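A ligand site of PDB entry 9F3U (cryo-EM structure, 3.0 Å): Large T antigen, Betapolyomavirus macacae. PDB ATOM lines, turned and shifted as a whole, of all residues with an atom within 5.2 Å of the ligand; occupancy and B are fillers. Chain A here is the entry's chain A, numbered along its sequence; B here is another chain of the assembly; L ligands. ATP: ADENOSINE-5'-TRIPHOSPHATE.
An oxygen (O2B) of the ligand lies within hydrogen-bond range of the side-chain hydroxyl of Thr 168 (2.5 Å). The backbone NH (N) of Gly 166 is in hydrogen-bond range of an oxygen (O3A) of the ligand, 2.9 Å away. The backbone NH (N) of Lys 285 sits at hydrogen-bond distance from a nitrogen (N1) of the ligand (2.9 Å). NH2 of Arg 275 of chain B is in salt-bridge range of O1G of the ligand (2.7 Å). N of Thr 168 is in hydrogen-bond range of O2B of the ligand, at 2.7 Å. An oxygen (O1A) of the ligand is in hydrogen-bond range of the side-chain hydroxyl (OG1) of Thr 169 (2.5 Å). N of Ser 165 sits at hydrogen-bond distance from O1B of the ligand (2.9 Å). O of Pro 162 lies close to O1B of the ligand, 2.8 Å away. The backbone NH of Asp 164 sits at hydrogen-bond distance from an oxygen (O3B) of the ligand (2.9 Å). O1A of the ligand is in hydrogen-bond range of N of Thr 169 (2.6 Å). The side-chain amino group of Lys 153 of chain B is in salt-bridge range of an oxygen (O2A) of the ligand (2.8 Å). The side-chain amino group of Lys 167 is in salt-bridge range of an oxygen (O3G) of the ligand, at 2.7 Å.
Residues that only touch the ligand: Ile 163 (3.2 Å), Pro 284 (3.4 Å), Leu 292 (3.6 Å), Asn 264 (3.7 Å), Asp 237 of chain B (3.7 Å), Asp 209 (3.8 Å), Lys 289 (3.8 Å) and Leu 132 (3.96 Å). Hydrophobic or aromatic side chains that line the ligand: Leu 132, Ile 163 and Leu 292. 18 residues have an atom within 4 Å of the ligand: Leu 132, Pro 162, Ile 163, Asp 164, Ser 165, Gly 166, Lys 167, Thr 168, Thr 169, Asp 209, Asn 264, Pro 284, Lys 285, Lys 289, Leu 292, Lys 153 of chain B, Asp 237 of chain B and Arg 275 of chain B.
The side-chain amino group (NZ) of Lys 167 lies within hydrogen-bond range of the side-chain amide oxygen (OD1) of Asn 264, at 2.9 Å. NZ of Lys 153 of chain B lies within salt-bridge range of OD2 of Asp 237 of chain B. The backbone carbonyl oxygen (O) of Pro 162 sits at hydrogen-bond distance from the side-chain hydroxyl (OG) of Ser 165, 3.1 Å away. OD1 of Asn 264 sits close to O of Gly 161 (2.7 Å). The side-chain hydroxyl (OG) of Ser 165 sits at hydrogen-bond distance from the backbone carbonyl oxygen (O) of Ile 163. NE of Arg 275 of chain B is in salt-bridge range of OD1 of Asp 237 of chain B, 2.6 Å away. The side-chain amino group (NZ) of Lys 167 lies within hydrogen-bond range of the backbone carbonyl oxygen (O) of Pro 162 (2.7 Å). NZ of Lys 285 is in hydrogen-bond range of O of Arg 283 (2.8 Å).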
ATOM      1  N   LEU A 132      30.728  31.964  22.767  1.00  0.00           N
ATOM      2  CA  LEU A 132      29.482  31.522  22.153  1.00  0.00           C
ATOM      3  C   LEU A 132      28.966  32.522  21.115  1.00  0.00           C
ATOM      4  O   LEU A 132      28.459  32.119  20.060  1.00  0.00           O
ATOM      5  CB  LEU A 132      28.429  31.289  23.226  1.00  0.00           C
ATOM      6  CG  LEU A 132      27.020  30.940  22.723  1.00  0.00           C
ATOM      7  CD1 LEU A 132      27.027  29.609  21.972  1.00  0.00           C
ATOM      8  CD2 LEU A 132      26.051  30.870  23.896  1.00  0.00           C
ATOM      9  N   GLY A 161      15.755  30.474  16.880  1.00  0.00           N
ATOM     10  CA  GLY A 161      16.714  29.533  16.306  1.00  0.00           C
ATOM     11  C   GLY A 161      16.395  28.063  16.480  1.00  0.00           C
ATOM     12  O   GLY A 161      15.468  27.677  17.188  1.00  0.00           O
ATOM     13  N   PRO A 162      17.186  27.203  15.816  1.00  0.00           N
ATOM     14  CA  PRO A 162      16.916  25.757  15.826  1.00  0.00           C
ATOM     15  C   PRO A 162      17.023  25.170  17.229  1.00  0.00           C
ATOM     16  O   PRO A 162      17.489  25.804  18.175  1.00  0.00           O
ATOM     17  CB  PRO A 162      17.990  25.161  14.907  1.00  0.00           C
ATOM     18  CG  PRO A 162      18.714  26.330  14.294  1.00  0.00           C
ATOM     19  CD  PRO A 162      18.444  27.530  15.134  1.00  0.00           C
ATOM     20  N   ILE A 163      16.585  23.907  17.358  1.00  0.00           N
ATOM     21  CA  ILE A 163      16.867  23.147  18.569  1.00  0.00           C
ATOM     22  C   ILE A 163      18.369  23.010  18.809  1.00  0.00           C
ATOM     23  O   ILE A 163      19.173  23.047  17.873  1.00  0.00           O
ATOM     24  CB  ILE A 163      16.212  21.759  18.543  1.00  0.00           C
ATOM     25  CG1 ILE A 163      16.815  20.868  17.451  1.00  0.00           C
ATOM     26  CG2 ILE A 163      14.703  21.886  18.375  1.00  0.00           C
ATOM     27  CD1 ILE A 163      16.298  19.429  17.482  1.00  0.00           C
ATOM     28  N   ASP A 164      18.721  22.849  20.077  1.00  0.00           N
ATOM     29  CA  ASP A 164      20.111  22.617  20.491  1.00  0.00           C
ATOM     30  C   ASP A 164      21.057  23.640  19.875  1.00  0.00           C
ATOM     31  O   ASP A 164      22.181  23.328  19.474  1.00  0.00           O
ATOM     32  CB  ASP A 164      20.535  21.189  20.162  1.00  0.00           C
ATOM     33  CG  ASP A 164      19.681  20.161  20.868  1.00  0.00           C
ATOM     34  OD1 ASP A 164      18.945  20.553  21.801  1.00  0.00           O
ATOM     35  OD2 ASP A 164      19.747  18.966  20.513  1.00  0.00           O
ATOM     36  N   SER A 165      20.587  24.883  19.793  1.00  0.00           N
ATOM     37  CA  SER A 165      21.357  25.986  19.239  1.00  0.00           C
ATOM     38  C   SER A 165      21.615  27.049  20.305  1.00  0.00           C
ATOM     39  O   SER A 165      22.080  28.145  19.975  1.00  0.00           O
ATOM     40  CB  SER A 165      20.638  26.580  18.031  1.00  0.00           C
ATOM     41  OG  SER A 165      20.399  25.573  17.048  1.00  0.00           O
ATOM     42  N   GLY A 166      21.311  26.736  21.565  1.00  0.00           N
ATOM     43  CA  GLY A 166      21.851  27.441  22.713  1.00  0.00           C
ATOM     44  C   GLY A 166      20.977  28.561  23.255  1.00  0.00           C
ATOM     45  O   GLY A 166      21.283  29.082  24.327  1.00  0.00           O
ATOM     46  N   LYS A 167      19.918  28.934  22.549  1.00  0.00           N
ATOM     47  CA  LYS A 167      19.085  30.038  23.011  1.00  0.00           C
ATOM     48  C   LYS A 167      18.609  29.828  24.441  1.00  0.00           C
ATOM     49  O   LYS A 167      18.677  30.743  25.264  1.00  0.00           O
ATOM     50  CB  LYS A 167      17.921  30.257  22.033  1.00  0.00           C
ATOM     51  CG  LYS A 167      17.053  29.041  21.806  1.00  0.00           C
ATOM     52  CD  LYS A 167      16.000  29.256  20.728  1.00  0.00           C
ATOM     53  CE  LYS A 167      15.093  28.036  20.602  1.00  0.00           C
ATOM     54  NZ  LYS A 167      15.773  26.902  19.913  1.00  0.00           N
ATOM     55  N   THR A 168      18.152  28.621  24.775  1.00  0.00           N
ATOM     56  CA  THR A 168      17.767  28.334  26.153  1.00  0.00           C
ATOM     57  C   THR A 168      18.939  28.501  27.103  1.00  0.00           C
ATOM     58  O   THR A 168      18.789  29.072  28.192  1.00  0.00           O
ATOM     59  CB  THR A 168      17.210  26.911  26.262  1.00  0.00           C
ATOM     60  OG1 THR A 168      16.145  26.745  25.321  1.00  0.00           O
ATOM     61  CG2 THR A 168      16.687  26.663  27.666  1.00  0.00           C
ATOM     62  N   THR A 169      20.116  28.006  26.724  1.00  0.00           N
ATOM     63  CA  THR A 169      21.297  28.155  27.566  1.00  0.00           C
ATOM     64  C   THR A 169      21.531  29.612  27.958  1.00  0.00           C
ATOM     65  O   THR A 169      21.809  29.916  29.118  1.00  0.00           O
ATOM     66  CB  THR A 169      22.517  27.618  26.819  1.00  0.00           C
ATOM     67  OG1 THR A 169      22.250  26.286  26.361  1.00  0.00           O
ATOM     68  CG2 THR A 169      23.741  27.614  27.710  1.00  0.00           C
ATOM     69  N   LEU A 170      21.414  30.510  26.991  1.00  0.00           N
ATOM     70  CA  LEU A 170      21.595  31.932  27.277  1.00  0.00           C
ATOM     71  C   LEU A 170      20.441  32.505  28.099  1.00  0.00           C
ATOM     72  O   LEU A 170      20.652  33.256  29.042  1.00  0.00           O
ATOM     73  CB  LEU A 170      21.747  32.684  25.963  1.00  0.00           C
ATOM     74  CG  LEU A 170      21.979  34.182  26.068  1.00  0.00           C
ATOM     75  CD1 LEU A 170      23.217  34.468  26.892  1.00  0.00           C
ATOM     76  CD2 LEU A 170      22.115  34.756  24.676  1.00  0.00           C
ATOM     77  N   ASP A 209       9.778  28.464  24.076  1.00  0.00           N
ATOM     78  CA  ASP A 209       9.684  27.581  22.906  1.00  0.00           C
ATOM     79  C   ASP A 209       8.266  27.488  22.331  1.00  0.00           C
ATOM     80  O   ASP A 209       7.724  26.409  22.106  1.00  0.00           O
ATOM     81  CB  ASP A 209      10.252  26.208  23.235  1.00  0.00           C
ATOM     82  CG  ASP A 209      11.693  26.291  23.720  1.00  0.00           C
ATOM     83  OD1 ASP A 209      12.357  27.298  23.430  1.00  0.00           O
ATOM     84  OD2 ASP A 209      12.151  25.347  24.399  1.00  0.00           O
ATOM     85  N   ASN A 264      11.600  27.827  17.967  1.00  0.00           N
ATOM     86  CA  ASN A 264      12.213  27.518  16.682  1.00  0.00           C
ATOM     87  C   ASN A 264      11.454  28.263  15.586  1.00  0.00           C
ATOM     88  O   ASN A 264      10.562  29.072  15.854  1.00  0.00           O
ATOM     89  CB  ASN A 264      12.249  26.005  16.477  1.00  0.00           C
ATOM     90  CG  ASN A 264      12.901  25.270  17.643  1.00  0.00           C
ATOM     91  OD1 ASN A 264      14.064  25.502  17.960  1.00  0.00           O
ATOM     92  ND2 ASN A 264      12.132  24.420  18.307  1.00  0.00           N
ATOM     93  N   PHE A 282      21.037  32.353  17.130  1.00  0.00           N
ATOM     94  CA  PHE A 282      22.383  31.904  16.806  1.00  0.00           C
ATOM     95  C   PHE A 282      22.381  30.382  16.662  1.00  0.00           C
ATOM     96  O   PHE A 282      21.550  29.691  17.266  1.00  0.00           O
ATOM     97  CB  PHE A 282      23.373  32.380  17.880  1.00  0.00           C
ATOM     98  CG  PHE A 282      22.983  31.978  19.282  1.00  0.00           C
ATOM     99  CD1 PHE A 282      22.027  32.704  19.973  1.00  0.00           C
ATOM    100  CD2 PHE A 282      23.614  30.924  19.923  1.00  0.00           C
ATOM    101  CE1 PHE A 282      21.675  32.359  21.268  1.00  0.00           C
ATOM    102  CE2 PHE A 282      23.258  30.571  21.219  1.00  0.00           C
ATOM    103  CZ  PHE A 282      22.289  31.288  21.891  1.00  0.00           C
ATOM    104  N   ARG A 283      23.289  29.867  15.844  1.00  0.00           N
ATOM    105  CA  ARG A 283      23.166  28.510  15.318  1.00  0.00           C
ATOM    106  C   ARG A 283      24.493  27.765  15.342  1.00  0.00           C
ATOM    107  O   ARG A 283      25.564  28.388  15.259  1.00  0.00           O
ATOM    108  CB  ARG A 283      22.526  28.536  13.928  1.00  0.00           C
ATOM    109  CG  ARG A 283      21.255  29.400  13.989  1.00  0.00           C
ATOM    110  CD  ARG A 283      20.324  29.372  12.778  1.00  0.00           C
ATOM    111  NE  ARG A 283      19.198  30.269  13.056  1.00  0.00           N
ATOM    112  CZ  ARG A 283      18.099  30.385  12.333  1.00  0.00           C
ATOM    113  NH1 ARG A 283      17.930  29.691  11.211  1.00  0.00           N
ATOM    114  NH2 ARG A 283      17.141  31.206  12.740  1.00  0.00           N
ATOM    115  N   PRO A 284      24.459  26.430  15.458  1.00  0.00           N
ATOM    116  CA  PRO A 284      25.544  25.664  16.081  1.00  0.00           C
ATOM    117  C   PRO A 284      26.961  25.868  15.544  1.00  0.00           C
ATOM    118  O   PRO A 284      27.186  25.993  14.338  1.00  0.00           O
ATOM    119  CB  PRO A 284      25.097  24.211  15.881  1.00  0.00           C
ATOM    120  CG  PRO A 284      23.607  24.298  15.889  1.00  0.00           C
ATOM    121  CD  PRO A 284      23.309  25.572  15.148  1.00  0.00           C
ATOM    122  N   LYS A 285      27.920  25.881  16.474  1.00  0.00           N
ATOM    123  CA  LYS A 285      29.369  25.961  16.274  1.00  0.00           C
ATOM    124  C   LYS A 285      30.005  24.669  16.774  1.00  0.00           C
ATOM    125  O   LYS A 285      30.451  24.563  17.923  1.00  0.00           O
ATOM    126  CB  LYS A 285      29.939  27.167  16.998  1.00  0.00           C
ATOM    127  CG  LYS A 285      29.936  28.438  16.165  1.00  0.00           C
ATOM    128  CD  LYS A 285      28.552  28.749  15.620  1.00  0.00           C
ATOM    129  CE  LYS A 285      28.498  30.161  15.052  1.00  0.00           C
ATOM    130  NZ  LYS A 285      27.251  30.387  14.286  1.00  0.00           N
ATOM    131  N   ASP A 286      30.049  23.676  15.879  1.00  0.00           N
ATOM    132  CA  ASP A 286      30.363  22.290  16.220  1.00  0.00           C
ATOM    133  C   ASP A 286      31.609  22.102  17.103  1.00  0.00           C
ATOM    134  O   ASP A 286      31.626  21.210  17.960  1.00  0.00           O
ATOM    135  CB  ASP A 286      30.556  21.512  14.925  1.00  0.00           C
ATOM    136  CG  ASP A 286      30.927  20.069  15.173  1.00  0.00           C
ATOM    137  OD1 ASP A 286      30.184  19.368  15.889  1.00  0.00           O
ATOM    138  OD2 ASP A 286      31.981  19.629  14.647  1.00  0.00           O
ATOM    139  N   LEU A 288      32.587  23.861  19.580  1.00  0.00           N
ATOM    140  CA  LEU A 288      32.173  23.981  20.968  1.00  0.00           C
ATOM    141  C   LEU A 288      31.610  22.667  21.487  1.00  0.00           C
ATOM    142  O   LEU A 288      31.831  22.307  22.649  1.00  0.00           O
ATOM    143  CB  LEU A 288      31.111  25.072  21.101  1.00  0.00           C
ATOM    144  CG  LEU A 288      31.521  26.467  20.633  1.00  0.00           C
ATOM    145  CD1 LEU A 288      30.375  27.443  20.871  1.00  0.00           C
ATOM    146  CD2 LEU A 288      32.772  26.934  21.374  1.00  0.00           C
ATOM    147  N   LYS A 289      30.896  21.940  20.634  1.00  0.00           N
ATOM    148  CA  LYS A 289      30.356  20.644  21.030  1.00  0.00           C
ATOM    149  C   LYS A 289      31.483  19.693  21.444  1.00  0.00           C
ATOM    150  O   LYS A 289      31.442  19.105  22.525  1.00  0.00           O
ATOM    151  CB  LYS A 289      29.550  20.081  19.875  1.00  0.00           C
ATOM    152  CG  LYS A 289      28.179  19.581  20.288  1.00  0.00           C
ATOM    153  CD  LYS A 289      27.359  19.138  19.088  1.00  0.00           C
ATOM    154  CE  LYS A 289      25.966  18.694  19.524  1.00  0.00           C
ATOM    155  NZ  LYS A 289      25.144  18.225  18.377  1.00  0.00           N
ATOM    156  N   LEU A 292      32.784  20.893  24.865  1.00  0.00           N
ATOM    157  CA  LEU A 292      31.931  20.438  25.964  1.00  0.00           C
ATOM    158  C   LEU A 292      32.169  18.968  26.246  1.00  0.00           C
ATOM    159  O   LEU A 292      32.377  18.546  27.386  1.00  0.00           O
ATOM    160  CB  LEU A 292      30.471  20.665  25.622  1.00  0.00           C
ATOM    161  CG  LEU A 292      29.982  22.107  25.587  1.00  0.00           C
ATOM    162  CD1 LEU A 292      28.547  22.140  25.087  1.00  0.00           C
ATOM    163  CD2 LEU A 292      30.061  22.739  26.959  1.00  0.00           C
ATOM    164  N   LEU A 299      29.169  21.319  32.108  1.00  0.00           N
ATOM    165  CA  LEU A 299      27.753  20.982  32.118  1.00  0.00           C
ATOM    166  C   LEU A 299      27.349  20.300  33.414  1.00  0.00           C
ATOM    167  O   LEU A 299      26.287  20.594  33.968  1.00  0.00           O
ATOM    168  CB  LEU A 299      27.427  20.084  30.931  1.00  0.00           C
ATOM    169  CG  LEU A 299      27.139  20.849  29.649  1.00  0.00           C
ATOM    170  CD1 LEU A 299      27.220  19.912  28.455  1.00  0.00           C
ATOM    171  CD2 LEU A 299      25.760  21.476  29.720  1.00  0.00           C
ATOM    172  N   LYS B 153      19.205  18.330  29.825  1.00  0.00           N
ATOM    173  CA  LYS B 153      18.947  17.767  28.496  1.00  0.00           C
ATOM    174  C   LYS B 153      19.746  16.494  28.216  1.00  0.00           C
ATOM    175  O   LYS B 153      19.909  16.105  27.054  1.00  0.00           O
ATOM    176  CB  LYS B 153      19.184  18.829  27.405  1.00  0.00           C
ATOM    177  CG  LYS B 153      18.598  18.462  26.023  1.00  0.00           C
ATOM    178  CD  LYS B 153      18.705  19.584  24.987  1.00  0.00           C
ATOM    179  CE  LYS B 153      17.623  20.656  25.162  1.00  0.00           C
ATOM    180  NZ  LYS B 153      17.684  21.746  24.149  1.00  0.00           N
ATOM    181  N   ASP B 237      14.065  18.836  29.408  1.00  0.00           N
ATOM    182  CA  ASP B 237      15.416  19.384  29.393  1.00  0.00           C
ATOM    183  C   ASP B 237      15.883  19.778  30.773  1.00  0.00           C
ATOM    184  O   ASP B 237      17.065  19.612  31.109  1.00  0.00           O
ATOM    185  CB  ASP B 237      15.437  20.600  28.476  1.00  0.00           C
ATOM    186  CG  ASP B 237      15.160  20.240  27.041  1.00  0.00           C
ATOM    187  OD1 ASP B 237      15.380  19.075  26.661  1.00  0.00           O
ATOM    188  OD2 ASP B 237      14.714  21.125  26.279  1.00  0.00           O
ATOM    189  N   SER B 239      16.510  22.623  31.958  1.00  0.00           N
ATOM    190  CA  SER B 239      17.384  23.783  32.020  1.00  0.00           C
ATOM    191  C   SER B 239      16.816  24.892  32.884  1.00  0.00           C
ATOM    192  O   SER B 239      17.562  25.779  33.303  1.00  0.00           O
ATOM    193  CB  SER B 239      17.658  24.321  30.622  1.00  0.00           C
ATOM    194  OG  SER B 239      18.377  23.379  29.858  1.00  0.00           O
ATOM    195  N   ARG B 275      16.052  14.494  22.832  1.00  0.00           N
ATOM    196  CA  ARG B 275      16.091  14.693  24.278  1.00  0.00           C
ATOM    197  C   ARG B 275      16.322  13.422  25.080  1.00  0.00           C
ATOM    198  O   ARG B 275      16.687  13.517  26.255  1.00  0.00           O
ATOM    199  CB  ARG B 275      14.814  15.400  24.712  1.00  0.00           C
ATOM    200  CG  ARG B 275      14.819  16.802  24.175  1.00  0.00           C
ATOM    201  CD  ARG B 275      13.580  17.584  24.468  1.00  0.00           C
ATOM    202  NE  ARG B 275      13.901  19.001  24.482  1.00  0.00           N
ATOM    203  CZ  ARG B 275      14.256  19.722  23.423  1.00  0.00           C
ATOM    204  NH1 ARG B 275      14.206  19.228  22.194  1.00  0.00           N
ATOM    205  NH2 ARG B 275      14.664  20.971  23.598  1.00  0.00           N
HETATM  206  PG  ATP L   1      15.645  23.863  22.185  1.00  0.00           P
HETATM  207  O1G ATP L   1      15.472  22.550  21.503  1.00  0.00           O
HETATM  208  O2G ATP L   1      15.418  23.633  23.676  1.00  0.00           O
HETATM  209  O3G ATP L   1      14.853  24.968  21.508  1.00  0.00           O
HETATM  210  PB  ATP L   1      17.992  25.605  22.218  1.00  0.00           P
HETATM  211  O1B ATP L   1      18.209  26.196  20.883  1.00  0.00           O
HETATM  212  O2B ATP L   1      17.362  26.599  23.176  1.00  0.00           O
HETATM  213  O3B ATP L   1      17.145  24.315  22.080  1.00  0.00           O
HETATM  214  PA  ATP L   1      19.876  24.888  24.301  1.00  0.00           P
HETATM  215  O1A ATP L   1      20.265  26.167  24.916  1.00  0.00           O
HETATM  216  O2A ATP L   1      18.863  24.093  25.121  1.00  0.00           O
HETATM  217  O3A ATP L   1      19.335  25.072  22.861  1.00  0.00           O
HETATM  218  O5' ATP L   1      21.193  24.047  24.146  1.00  0.00           O
HETATM  219  C5' ATP L   1      21.175  22.619  24.263  1.00  0.00           C
HETATM  220  C4' ATP L   1      22.520  22.081  23.839  1.00  0.00           C
HETATM  221  O4' ATP L   1      22.779  22.455  22.471  1.00  0.00           O
HETATM  222  C3' ATP L   1      23.653  22.762  24.584  1.00  0.00           C
HETATM  223  O3' ATP L   1      23.810  22.205  25.872  1.00  0.00           O
HETATM  224  C2' ATP L   1      24.832  22.449  23.669  1.00  0.00           C
HETATM  225  O2' ATP L   1      25.262  21.131  23.971  1.00  0.00           O
HETATM  226  C1' ATP L   1      24.192  22.475  22.279  1.00  0.00           C
HETATM  227  N9  ATP L   1      24.506  23.717  21.579  1.00  0.00           N
HETATM  228  C8  ATP L   1      23.845  24.906  21.646  1.00  0.00           C
HETATM  229  N7  ATP L   1      24.386  25.854  20.921  1.00  0.00           N
HETATM  230  C5  ATP L   1      25.505  25.253  20.375  1.00  0.00           C
HETATM  231  C6  ATP L   1      26.518  25.726  19.514  1.00  0.00           C
HETATM  232  N6  ATP L   1      26.575  26.974  19.046  1.00  0.00           N
HETATM  233  N1  ATP L   1      27.498  24.859  19.163  1.00  0.00           N
HETATM  234  C2  ATP L   1      27.450  23.608  19.631  1.00  0.00           C
HETATM  235  N3  ATP L   1      26.546  23.051  20.441  1.00  0.00           N
HETATM  236  C4  ATP L   1      25.592  23.926  20.771  1.00  0.00           C
